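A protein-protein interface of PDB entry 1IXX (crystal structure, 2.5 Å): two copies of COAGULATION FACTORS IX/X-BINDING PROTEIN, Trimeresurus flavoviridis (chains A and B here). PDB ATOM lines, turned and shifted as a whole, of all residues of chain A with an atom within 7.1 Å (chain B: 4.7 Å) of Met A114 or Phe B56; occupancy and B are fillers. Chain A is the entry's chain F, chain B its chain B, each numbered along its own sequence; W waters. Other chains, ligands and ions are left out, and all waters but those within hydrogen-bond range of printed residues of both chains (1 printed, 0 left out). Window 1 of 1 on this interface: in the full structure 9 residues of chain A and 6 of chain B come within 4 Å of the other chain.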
ATOM      1  N   SER A  18       0.745  -4.448 -26.958  1.00  0.00           N
ATOM      2  CA  SER A  18      -0.602  -4.647 -27.506  1.00  0.00           C
ATOM      3  C   SER A  18      -1.362  -5.904 -27.117  1.00  0.00           C
ATOM      4  O   SER A  18      -2.545  -5.823 -26.827  1.00  0.00           O
ATOM      5  CB  SER A  18      -0.585  -4.569 -29.032  1.00  0.00           C
ATOM      6  OG  SER A  18      -0.919  -3.267 -29.468  1.00  0.00           O
ATOM      7  N   GLU A  19      -0.714  -7.064 -27.161  1.00  0.00           N
ATOM      8  CA  GLU A  19      -1.391  -8.317 -26.834  1.00  0.00           C
ATOM      9  C   GLU A  19      -1.899  -8.404 -25.404  1.00  0.00           C
ATOM     10  O   GLU A  19      -1.119  -8.391 -24.454  1.00  0.00           O
ATOM     11  CB  GLU A  19      -0.506  -9.518 -27.159  1.00  0.00           C
ATOM     12  CG  GLU A  19      -0.770 -10.128 -28.529  1.00  0.00           C
ATOM     13  CD  GLU A  19      -2.128 -10.821 -28.620  1.00  0.00           C
ATOM     14  OE1 GLU A  19      -2.279 -11.922 -28.040  1.00  0.00           O
ATOM     15  OE2 GLU A  19      -3.045 -10.267 -29.273  1.00  0.00           O
ATOM     16  N   PRO A  20      -3.228  -8.483 -25.236  1.00  0.00           N
ATOM     17  CA  PRO A  20      -3.886  -8.575 -23.934  1.00  0.00           C
ATOM     18  C   PRO A  20      -3.535  -9.873 -23.227  1.00  0.00           C
ATOM     19  O   PRO A  20      -3.647 -10.948 -23.809  1.00  0.00           O
ATOM     20  CB  PRO A  20      -5.365  -8.545 -24.306  1.00  0.00           C
ATOM     21  CG  PRO A  20      -5.378  -7.751 -25.563  1.00  0.00           C
ATOM     22  CD  PRO A  20      -4.234  -8.366 -26.300  1.00  0.00           C
ATOM     23  N   LYS A  21      -3.144  -9.762 -21.961  1.00  0.00           N
ATOM     24  CA  LYS A  21      -2.775 -10.913 -21.144  1.00  0.00           C
ATOM     25  C   LYS A  21      -3.284 -10.726 -19.722  1.00  0.00           C
ATOM     26  O   LYS A  21      -3.685  -9.626 -19.331  1.00  0.00           O
ATOM     27  CB  LYS A  21      -1.257 -11.035 -21.082  1.00  0.00           C
ATOM     28  CG  LYS A  21      -0.601 -11.471 -22.368  1.00  0.00           C
ATOM     29  CD  LYS A  21       0.851 -11.049 -22.386  1.00  0.00           C
ATOM     30  CE  LYS A  21       1.614 -11.766 -23.469  1.00  0.00           C
ATOM     31  NZ  LYS A  21       1.885 -13.169 -23.041  1.00  0.00           N
ATOM     32  N   ASN A  22      -3.319 -11.808 -18.956  1.00  0.00           N
ATOM     33  CA  ASN A  22      -3.727 -11.679 -17.572  1.00  0.00           C
ATOM     34  C   ASN A  22      -2.496 -11.112 -16.837  1.00  0.00           C
ATOM     35  O   ASN A  22      -1.406 -11.033 -17.420  1.00  0.00           O
ATOM     36  CB  ASN A  22      -4.241 -13.018 -16.986  1.00  0.00           C
ATOM     37  CG  ASN A  22      -3.183 -14.122 -16.941  1.00  0.00           C
ATOM     38  OD1 ASN A  22      -1.985 -13.872 -16.985  1.00  0.00           O
ATOM     39  ND2 ASN A  22      -3.640 -15.351 -16.817  1.00  0.00           N
ATOM     40  N   TRP A  23      -2.658 -10.692 -15.585  1.00  0.00           N
ATOM     41  CA  TRP A  23      -1.542 -10.113 -14.837  1.00  0.00           C
ATOM     42  C   TRP A  23      -0.302 -10.999 -14.789  1.00  0.00           C
ATOM     43  O   TRP A  23       0.789 -10.566 -15.159  1.00  0.00           O
ATOM     44  CB  TRP A  23      -1.964  -9.763 -13.408  1.00  0.00           C
ATOM     45  CG  TRP A  23      -0.960  -8.903 -12.711  1.00  0.00           C
ATOM     46  CD1 TRP A  23      -0.940  -7.544 -12.676  1.00  0.00           C
ATOM     47  CD2 TRP A  23       0.208  -9.342 -12.003  1.00  0.00           C
ATOM     48  NE1 TRP A  23       0.169  -7.106 -12.001  1.00  0.00           N
ATOM     49  CE2 TRP A  23       0.894  -8.187 -11.577  1.00  0.00           C
ATOM     50  CE3 TRP A  23       0.745 -10.600 -11.693  1.00  0.00           C
ATOM     51  CZ2 TRP A  23       2.089  -8.247 -10.860  1.00  0.00           C
ATOM     52  CZ3 TRP A  23       1.930 -10.660 -10.983  1.00  0.00           C
ATOM     53  CH2 TRP A  23       2.591  -9.485 -10.575  1.00  0.00           C
ATOM     54  N   ASP A  25       0.800 -13.631 -16.571  1.00  0.00           N
ATOM     55  CA  ASP A  25       1.470 -13.773 -17.851  1.00  0.00           C
ATOM     56  C   ASP A  25       2.189 -12.515 -18.263  1.00  0.00           C
ATOM     57  O   ASP A  25       3.325 -12.583 -18.728  1.00  0.00           O
ATOM     58  CB  ASP A  25       0.484 -14.183 -18.945  1.00  0.00           C
ATOM     59  CG  ASP A  25       0.031 -15.622 -18.809  1.00  0.00           C
ATOM     60  OD1 ASP A  25       0.613 -16.361 -17.980  1.00  0.00           O
ATOM     61  OD2 ASP A  25      -0.915 -16.013 -19.529  1.00  0.00           O
ATOM     62  N   SER A  62      -7.315   2.465 -23.691  1.00  0.00           N
ATOM     63  CA  SER A  62      -7.410   1.090 -23.233  1.00  0.00           C
ATOM     64  C   SER A  62      -7.007   1.036 -21.760  1.00  0.00           C
ATOM     65  O   SER A  62      -6.915   2.076 -21.114  1.00  0.00           O
ATOM     66  CB  SER A  62      -6.517   0.184 -24.086  1.00  0.00           C
ATOM     67  OG  SER A  62      -6.675  -1.178 -23.715  1.00  0.00           O
ATOM     68  N   ILE A  63      -6.816  -0.172 -21.229  1.00  0.00           N
ATOM     69  CA  ILE A  63      -6.437  -0.385 -19.830  1.00  0.00           C
ATOM     70  C   ILE A  63      -5.150  -1.211 -19.787  1.00  0.00           C
ATOM     71  O   ILE A  63      -4.965  -2.108 -20.609  1.00  0.00           O
ATOM     72  CB  ILE A  63      -7.574  -1.080 -19.049  1.00  0.00           C
ATOM     73  CG1 ILE A  63      -7.969  -2.403 -19.717  1.00  0.00           C
ATOM     74  CG2 ILE A  63      -8.790  -0.182 -19.019  1.00  0.00           C
ATOM     75  CD1 ILE A  63      -9.029  -3.162 -18.982  1.00  0.00           C
ATOM     76  N   PHE A  64      -4.253  -0.887 -18.854  1.00  0.00           N
ATOM     77  CA  PHE A  64      -2.951  -1.552 -18.750  1.00  0.00           C
ATOM     78  C   PHE A  64      -2.611  -1.949 -17.313  1.00  0.00           C
ATOM     79  O   PHE A  64      -2.877  -1.194 -16.371  1.00  0.00           O
ATOM     80  CB  PHE A  64      -1.829  -0.618 -19.267  1.00  0.00           C
ATOM     81  CG  PHE A  64      -2.117   0.026 -20.607  1.00  0.00           C
ATOM     82  CD1 PHE A  64      -3.108   0.993 -20.733  1.00  0.00           C
ATOM     83  CD2 PHE A  64      -1.413  -0.354 -21.739  1.00  0.00           C
ATOM     84  CE1 PHE A  64      -3.391   1.568 -21.960  1.00  0.00           C
ATOM     85  CE2 PHE A  64      -1.687   0.212 -22.972  1.00  0.00           C
ATOM     86  CZ  PHE A  64      -2.683   1.177 -23.086  1.00  0.00           C
ATOM     87  N   TRP A  65      -1.986  -3.114 -17.156  1.00  0.00           N
ATOM     88  CA  TRP A  65      -1.569  -3.615 -15.849  1.00  0.00           C
ATOM     89  C   TRP A  65      -0.326  -2.883 -15.347  1.00  0.00           C
ATOM     90  O   TRP A  65       0.538  -2.482 -16.134  1.00  0.00           O
ATOM     91  CB  TRP A  65      -1.178  -5.094 -15.927  1.00  0.00           C
ATOM     92  CG  TRP A  65      -2.263  -6.070 -16.216  1.00  0.00           C
ATOM     93  CD1 TRP A  65      -2.355  -6.894 -17.300  1.00  0.00           C
ATOM     94  CD2 TRP A  65      -3.380  -6.382 -15.377  1.00  0.00           C
ATOM     95  NE1 TRP A  65      -3.458  -7.707 -17.184  1.00  0.00           N
ATOM     96  CE2 TRP A  65      -4.106  -7.412 -16.013  1.00  0.00           C
ATOM     97  CE3 TRP A  65      -3.841  -5.889 -14.151  1.00  0.00           C
ATOM     98  CZ2 TRP A  65      -5.265  -7.959 -15.465  1.00  0.00           C
ATOM     99  CZ3 TRP A  65      -4.994  -6.430 -13.606  1.00  0.00           C
ATOM    100  CH2 TRP A  65      -5.694  -7.457 -14.265  1.00  0.00           C
ATOM    101  N   ARG A 109      -8.789  -4.838 -10.826  1.00  0.00           N
ATOM    102  CA  ARG A 109      -9.414  -5.722 -11.788  1.00  0.00           C
ATOM    103  C   ARG A 109      -8.951  -7.116 -11.383  1.00  0.00           C
ATOM    104  O   ARG A 109      -7.824  -7.271 -10.908  1.00  0.00           O
ATOM    105  CB  ARG A 109      -8.869  -5.366 -13.169  1.00  0.00           C
ATOM    106  CG  ARG A 109      -9.472  -6.087 -14.331  1.00  0.00           C
ATOM    107  CD  ARG A 109      -8.814  -5.594 -15.605  1.00  0.00           C
ATOM    108  NE  ARG A 109      -9.248  -6.325 -16.790  1.00  0.00           N
ATOM    109  CZ  ARG A 109     -10.496  -6.352 -17.241  1.00  0.00           C
ATOM    110  NH1 ARG A 109     -11.459  -5.694 -16.607  1.00  0.00           N
ATOM    111  NH2 ARG A 109     -10.778  -7.012 -18.350  1.00  0.00           N
ATOM    112  N   ALA A 110      -9.820  -8.116 -11.520  1.00  0.00           N
ATOM    113  CA  ALA A 110      -9.465  -9.494 -11.159  1.00  0.00           C
ATOM    114  C   ALA A 110      -8.277  -9.949 -12.011  1.00  0.00           C
ATOM    115  O   ALA A 110      -8.329  -9.894 -13.239  1.00  0.00           O
ATOM    116  CB  ALA A 110     -10.656 -10.413 -11.356  1.00  0.00           C
ATOM    117  N   CYS A 111      -7.219 -10.411 -11.356  1.00  0.00           N
ATOM    118  CA  CYS A 111      -5.987 -10.820 -12.038  1.00  0.00           C
ATOM    119  C   CYS A 111      -6.051 -11.800 -13.199  1.00  0.00           C
ATOM    120  O   CYS A 111      -5.108 -11.871 -14.000  1.00  0.00           O
ATOM    121  CB  CYS A 111      -5.001 -11.357 -11.028  1.00  0.00           C
ATOM    122  SG  CYS A 111      -4.846 -10.305  -9.575  1.00  0.00           S
ATOM    123  N   ARG A 112      -7.117 -12.594 -13.251  1.00  0.00           N
ATOM    124  CA  ARG A 112      -7.296 -13.582 -14.311  1.00  0.00           C
ATOM    125  C   ARG A 112      -7.787 -12.924 -15.591  1.00  0.00           C
ATOM    126  O   ARG A 112      -7.799 -13.543 -16.652  1.00  0.00           O
ATOM    127  CB  ARG A 112      -8.333 -14.622 -13.888  1.00  0.00           C
ATOM    128  CG  ARG A 112      -9.726 -14.034 -13.733  1.00  0.00           C
ATOM    129  CD  ARG A 112     -10.808 -15.084 -13.848  1.00  0.00           C
ATOM    130  NE  ARG A 112     -12.131 -14.509 -13.627  1.00  0.00           N
ATOM    131  CZ  ARG A 112     -13.205 -14.800 -14.353  1.00  0.00           C
ATOM    132  NH1 ARG A 112     -13.126 -15.660 -15.361  1.00  0.00           N
ATOM    133  NH2 ARG A 112     -14.371 -14.244 -14.062  1.00  0.00           N
ATOM    134  N   MET A 113      -8.237 -11.684 -15.479  1.00  0.00           N
ATOM    135  CA  MET A 113      -8.773 -10.984 -16.629  1.00  0.00           C
ATOM    136  C   MET A 113      -7.726 -10.382 -17.536  1.00  0.00           C
ATOM    137  O   MET A 113      -6.545 -10.312 -17.182  1.00  0.00           O
ATOM    138  CB  MET A 113      -9.785  -9.938 -16.177  1.00  0.00           C
ATOM    139  CG  MET A 113     -10.851 -10.533 -15.288  1.00  0.00           C
ATOM    140  SD  MET A 113     -12.459  -9.801 -15.543  1.00  0.00           S
ATOM    141  CE  MET A 113     -13.496 -11.085 -14.770  1.00  0.00           C
ATOM    142  N   MET A 114      -8.165 -10.000 -18.730  1.00  0.00           N
ATOM    143  CA  MET A 114      -7.293  -9.423 -19.739  1.00  0.00           C
ATOM    144  C   MET A 114      -7.120  -7.925 -19.576  1.00  0.00           C
ATOM    145  O   MET A 114      -7.972  -7.237 -19.014  1.00  0.00           O
ATOM    146  CB  MET A 114      -7.841  -9.704 -21.143  1.00  0.00           C
ATOM    147  CG  MET A 114      -8.028 -11.181 -21.472  1.00  0.00           C
ATOM    148  SD  MET A 114      -6.489 -12.092 -21.730  1.00  0.00           S
ATOM    149  CE  MET A 114      -6.404 -13.074 -20.252  1.00  0.00           C
ATOM    150  N   ALA A 115      -5.974  -7.449 -20.043  1.00  0.00           N
ATOM    151  CA  ALA A 115      -5.624  -6.037 -20.054  1.00  0.00           C
ATOM    152  C   ALA A 115      -4.322  -5.958 -20.817  1.00  0.00           C
ATOM    153  O   ALA A 115      -3.667  -6.978 -21.060  1.00  0.00           O
ATOM    154  CB  ALA A 115      -5.438  -5.494 -18.634  1.00  0.00           C
ATOM    155  N   GLN A 116      -4.011  -4.778 -21.324  1.00  0.00           N
ATOM    156  CA  GLN A 116      -2.745  -4.604 -22.012  1.00  0.00           C
ATOM    157  C   GLN A 116      -1.767  -4.259 -20.895  1.00  0.00           C
ATOM    158  O   GLN A 116      -2.147  -4.246 -19.722  1.00  0.00           O
ATOM    159  CB  GLN A 116      -2.826  -3.490 -23.036  1.00  0.00           C
ATOM    160  CG  GLN A 116      -3.820  -3.766 -24.122  1.00  0.00           C
ATOM    161  CD  GLN A 116      -3.764  -2.721 -25.182  1.00  0.00           C
ATOM    162  OE1 GLN A 116      -4.744  -2.036 -25.445  1.00  0.00           O
ATOM    163  NE2 GLN A 116      -2.591  -2.551 -25.774  1.00  0.00           N
ATOM    164  N   VAL B  52     -16.268 -11.936 -23.965  1.00  0.00           N
ATOM    165  CA  VAL B  52     -15.701 -10.663 -23.540  1.00  0.00           C
ATOM    166  C   VAL B  52     -14.188 -10.740 -23.678  1.00  0.00           C
ATOM    167  O   VAL B  52     -13.553  -9.819 -24.194  1.00  0.00           O
ATOM    168  CB  VAL B  52     -16.072 -10.331 -22.074  1.00  0.00           C
ATOM    169  CG1 VAL B  52     -15.355  -9.069 -21.625  1.00  0.00           C
ATOM    170  CG2 VAL B  52     -17.577 -10.138 -21.941  1.00  0.00           C
ATOM    171  N   LYS B  53     -13.634 -11.875 -23.258  1.00  0.00           N
ATOM    172  CA  LYS B  53     -12.199 -12.129 -23.321  1.00  0.00           C
ATOM    173  C   LYS B  53     -11.720 -12.157 -24.766  1.00  0.00           C
ATOM    174  O   LYS B  53     -10.712 -11.536 -25.091  1.00  0.00           O
ATOM    175  CB  LYS B  53     -11.875 -13.452 -22.619  1.00  0.00           C
ATOM    176  CG  LYS B  53     -10.414 -13.844 -22.608  1.00  0.00           C
ATOM    177  CD  LYS B  53     -10.216 -15.093 -21.769  1.00  0.00           C
ATOM    178  CE  LYS B  53      -8.765 -15.538 -21.770  1.00  0.00           C
ATOM    179  NZ  LYS B  53      -8.320 -15.982 -23.128  1.00  0.00           N
ATOM    180  N   LEU B  54     -12.459 -12.848 -25.631  1.00  0.00           N
ATOM    181  CA  LEU B  54     -12.117 -12.951 -27.053  1.00  0.00           C
ATOM    182  C   LEU B  54     -12.130 -11.548 -27.672  1.00  0.00           C
ATOM    183  O   LEU B  54     -11.206 -11.148 -28.382  1.00  0.00           O
ATOM    184  CB  LEU B  54     -13.140 -13.835 -27.775  1.00  0.00           C
ATOM    185  CG  LEU B  54     -12.783 -14.598 -29.059  1.00  0.00           C
ATOM    186  CD1 LEU B  54     -14.074 -14.915 -29.805  1.00  0.00           C
ATOM    187  CD2 LEU B  54     -11.851 -13.814 -29.966  1.00  0.00           C
ATOM    188  N   ALA B  55     -13.191 -10.806 -27.383  1.00  0.00           N
ATOM    189  CA  ALA B  55     -13.354  -9.451 -27.881  1.00  0.00           C
ATOM    190  C   ALA B  55     -12.184  -8.581 -27.451  1.00  0.00           C
ATOM    191  O   ALA B  55     -11.616  -7.865 -28.274  1.00  0.00           O
ATOM    192  CB  ALA B  55     -14.675  -8.867 -27.384  1.00  0.00           C
ATOM    193  N   PHE B  56     -11.793  -8.675 -26.178  1.00  0.00           N
ATOM    194  CA  PHE B  56     -10.676  -7.878 -25.669  1.00  0.00           C
ATOM    195  C   PHE B  56      -9.349  -8.287 -26.313  1.00  0.00           C
ATOM    196  O   PHE B  56      -8.611  -7.441 -26.825  1.00  0.00           O
ATOM    197  CB  PHE B  56     -10.556  -7.934 -24.127  1.00  0.00           C
ATOM    198  CG  PHE B  56      -9.715  -6.811 -23.564  1.00  0.00           C
ATOM    199  CD1 PHE B  56     -10.284  -5.564 -23.314  1.00  0.00           C
ATOM    200  CD2 PHE B  56      -8.335  -6.939 -23.455  1.00  0.00           C
ATOM    201  CE1 PHE B  56      -9.484  -4.463 -22.984  1.00  0.00           C
ATOM    202  CE2 PHE B  56      -7.537  -5.851 -23.126  1.00  0.00           C
ATOM    203  CZ  PHE B  56      -8.111  -4.610 -22.895  1.00  0.00           C
ATOM    204  N   GLN B  57      -9.071  -9.588 -26.312  1.00  0.00           N
ATOM    205  CA  GLN B  57      -7.844 -10.126 -26.890  1.00  0.00           C
ATOM    206  C   GLN B  57      -7.691  -9.783 -28.363  1.00  0.00           C
ATOM    207  O   GLN B  57      -6.576  -9.671 -28.866  1.00  0.00           O
ATOM    208  CB  GLN B  57      -7.796 -11.646 -26.750  1.00  0.00           C
ATOM    209  CG  GLN B  57      -7.707 -12.164 -25.334  1.00  0.00           C
ATOM    210  CD  GLN B  57      -7.421 -13.657 -25.303  1.00  0.00           C
ATOM    211  OE1 GLN B  57      -8.109 -14.447 -25.952  1.00  0.00           O
ATOM    212  NE2 GLN B  57      -6.393 -14.051 -24.561  1.00  0.00           N
ATOM    213  N   THR B  58      -8.810  -9.608 -29.049  1.00  0.00           N
ATOM    214  CA  THR B  58      -8.780  -9.312 -30.473  1.00  0.00           C
ATOM    215  C   THR B  58      -8.802  -7.828 -30.834  1.00  0.00           C
ATOM    216  O   THR B  58      -8.062  -7.400 -31.717  1.00  0.00           O
ATOM    217  CB  THR B  58      -9.944 -10.049 -31.211  1.00  0.00           C
ATOM    218  OG1 THR B  58      -9.955 -11.440 -30.841  1.00  0.00           O
ATOM    219  CG2 THR B  58      -9.787  -9.933 -32.711  1.00  0.00           C
ATOM    220  N   PHE B  59      -9.640  -7.040 -30.167  1.00  0.00           N
ATOM    221  CA  PHE B  59      -9.751  -5.625 -30.500  1.00  0.00           C
ATOM    222  C   PHE B  59      -9.544  -4.617 -29.371  1.00  0.00           C
ATOM    223  O   PHE B  59      -9.786  -3.416 -29.554  1.00  0.00           O
ATOM    224  CB  PHE B  59     -11.081  -5.376 -31.203  1.00  0.00           C
ATOM    225  CG  PHE B  59     -11.155  -5.982 -32.577  1.00  0.00           C
ATOM    226  CD1 PHE B  59     -10.185  -5.680 -33.536  1.00  0.00           C
ATOM    227  CD2 PHE B  59     -12.151  -6.890 -32.902  1.00  0.00           C
ATOM    228  CE1 PHE B  59     -10.212  -6.279 -34.787  1.00  0.00           C
ATOM    229  CE2 PHE B  59     -12.180  -7.491 -34.153  1.00  0.00           C
ATOM    230  CZ  PHE B  59     -11.208  -7.184 -35.093  1.00  0.00           C
ATOM    231  N   GLY B  60      -9.088  -5.104 -28.221  1.00  0.00           N
ATOM    232  CA  GLY B  60      -8.838  -4.233 -27.091  1.00  0.00           C
ATOM    233  C   GLY B  60     -10.055  -3.679 -26.385  1.00  0.00           C
ATOM    234  O   GLY B  60     -11.072  -4.351 -26.236  1.00  0.00           O
ATOM    235  N   HIS B  61      -9.935  -2.433 -25.952  1.00  0.00           N
ATOM    236  CA  HIS B  61     -10.973  -1.720 -25.215  1.00  0.00           C
ATOM    237  C   HIS B  61     -12.037  -1.127 -26.143  1.00  0.00           C
ATOM    238  O   HIS B  61     -11.831  -0.070 -26.731  1.00  0.00           O
ATOM    239  CB  HIS B  61     -10.292  -0.597 -24.411  1.00  0.00           C
ATOM    240  CG  HIS B  61     -11.194   0.121 -23.455  1.00  0.00           C
ATOM    241  ND1 HIS B  61     -12.284   0.861 -23.862  1.00  0.00           N
ATOM    242  CD2 HIS B  61     -11.173   0.197 -22.103  1.00  0.00           C
ATOM    243  CE1 HIS B  61     -12.901   1.350 -22.804  1.00  0.00           C
ATOM    244  NE2 HIS B  61     -12.247   0.961 -21.725  1.00  0.00           N
ATOM    245  N   SER B 101     -15.861  -4.515 -23.668  1.00  0.00           N
ATOM    246  CA  SER B 101     -14.842  -5.539 -23.461  1.00  0.00           C
ATOM    247  C   SER B 101     -14.106  -5.602 -22.119  1.00  0.00           C
ATOM    248  O   SER B 101     -13.258  -6.477 -21.922  1.00  0.00           O
ATOM    249  CB  SER B 101     -13.853  -5.577 -24.640  1.00  0.00           C
ATOM    250  OG  SER B 101     -13.481  -4.281 -25.074  1.00  0.00           O
HETATM  251  O   HOH W   1     -12.198  -8.529 -20.462  1.00  0.00           O
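The backbone carbonyl oxygen (O) of Met A114 is in hydrogen-bond range of the guanidinium group (NE) of Arg A109, 2.7 Å away.
The backbone NH (N) of Lys A21 sits at hydrogen-bond distance from the backbone carbonyl oxygen (O) of Ala A115, 3.0 Å away.
OG of Ser A62 is in hydrogen-bond range of OE1 of Gln A116 (2.7 Å).
The backbone carbonyl oxygen (O) of Ile A63 is in hydrogen-bond range of the backbone NH (N) of Gln A116, at 2.9 Å.
The side-chain amide nitrogen of Gln B57 sits close to the side-chain amino group of Lys B53 (3.1 Å).
Water W1 bridges the backbone carbonyl oxygen of Ser B101 and the guanidinium group of Arg A109.
The side-chain amide nitrogen of Gln B57 lies within hydrogen-bond range of the side-chain sulfur of Met A114, 3.4 Å away.
No position is printed for both chains.
Of the 11 pairs that touch across the chains among the printed residues, none has its exchanged pair printed and touching as well.
Of the 19 printed residues of chain A, 6 touch a printed residue of chain B.
Hydrophobic or aromatic side chains of chain A that line the printed part of chain B: Pro A20, Ile A63 and Met A114.
Among the printed residues, 11 pairs touch across the chains.
Among the printed residues, no Asp or Glu carboxylate lies within 4 Å of a Lys or Arg side-chain nitrogen of the other chain.
Met A114 touches just these residues of chain B: Lys B53, Phe B56 and Gln B57.
Of the printed residues of chain B, Glu A19 touches Gln B57 (3.6 Å).
Of the printed residues of chain B, Ile A63 touches Phe B56 (3.9 Å) and His B61 (3.9 Å).
Of the printed residues of chain B, Ala A115 touches Phe B56.
Of the printed residues of chain A, Lys B53 touches Met A114.
Leu B54 touches none of the printed residues of chain A.
The nearest printed residue of chain B that does not touch Met A114 is Ser B101 (6.1 Å).
The nearest residue of chain A that does not touch Phe B56 is Gln A116 (4.1 Å).
Glu A19 touches Gln B57.
Phe B56 touches Pro A20 (CD2 to CB, 3.5 Å).
Pro A20 touches Gln B57.
CZ of Phe B56 touches OG of Ser A62, 3.8 Å away.
CA of Ser A62 touches CB of His B61 (3.5 Å).
Ile A63 touches Phe B56.
Ile A63 touches His B61 (CG2 to CD2, 3.9 Å).
CE of Met A114 touches CE of Lys B53 (3.7 Å).
Phe B56 touches Met A114.
Ala A115 touches Phe B56 (CA to CE2, 3.6 Å).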
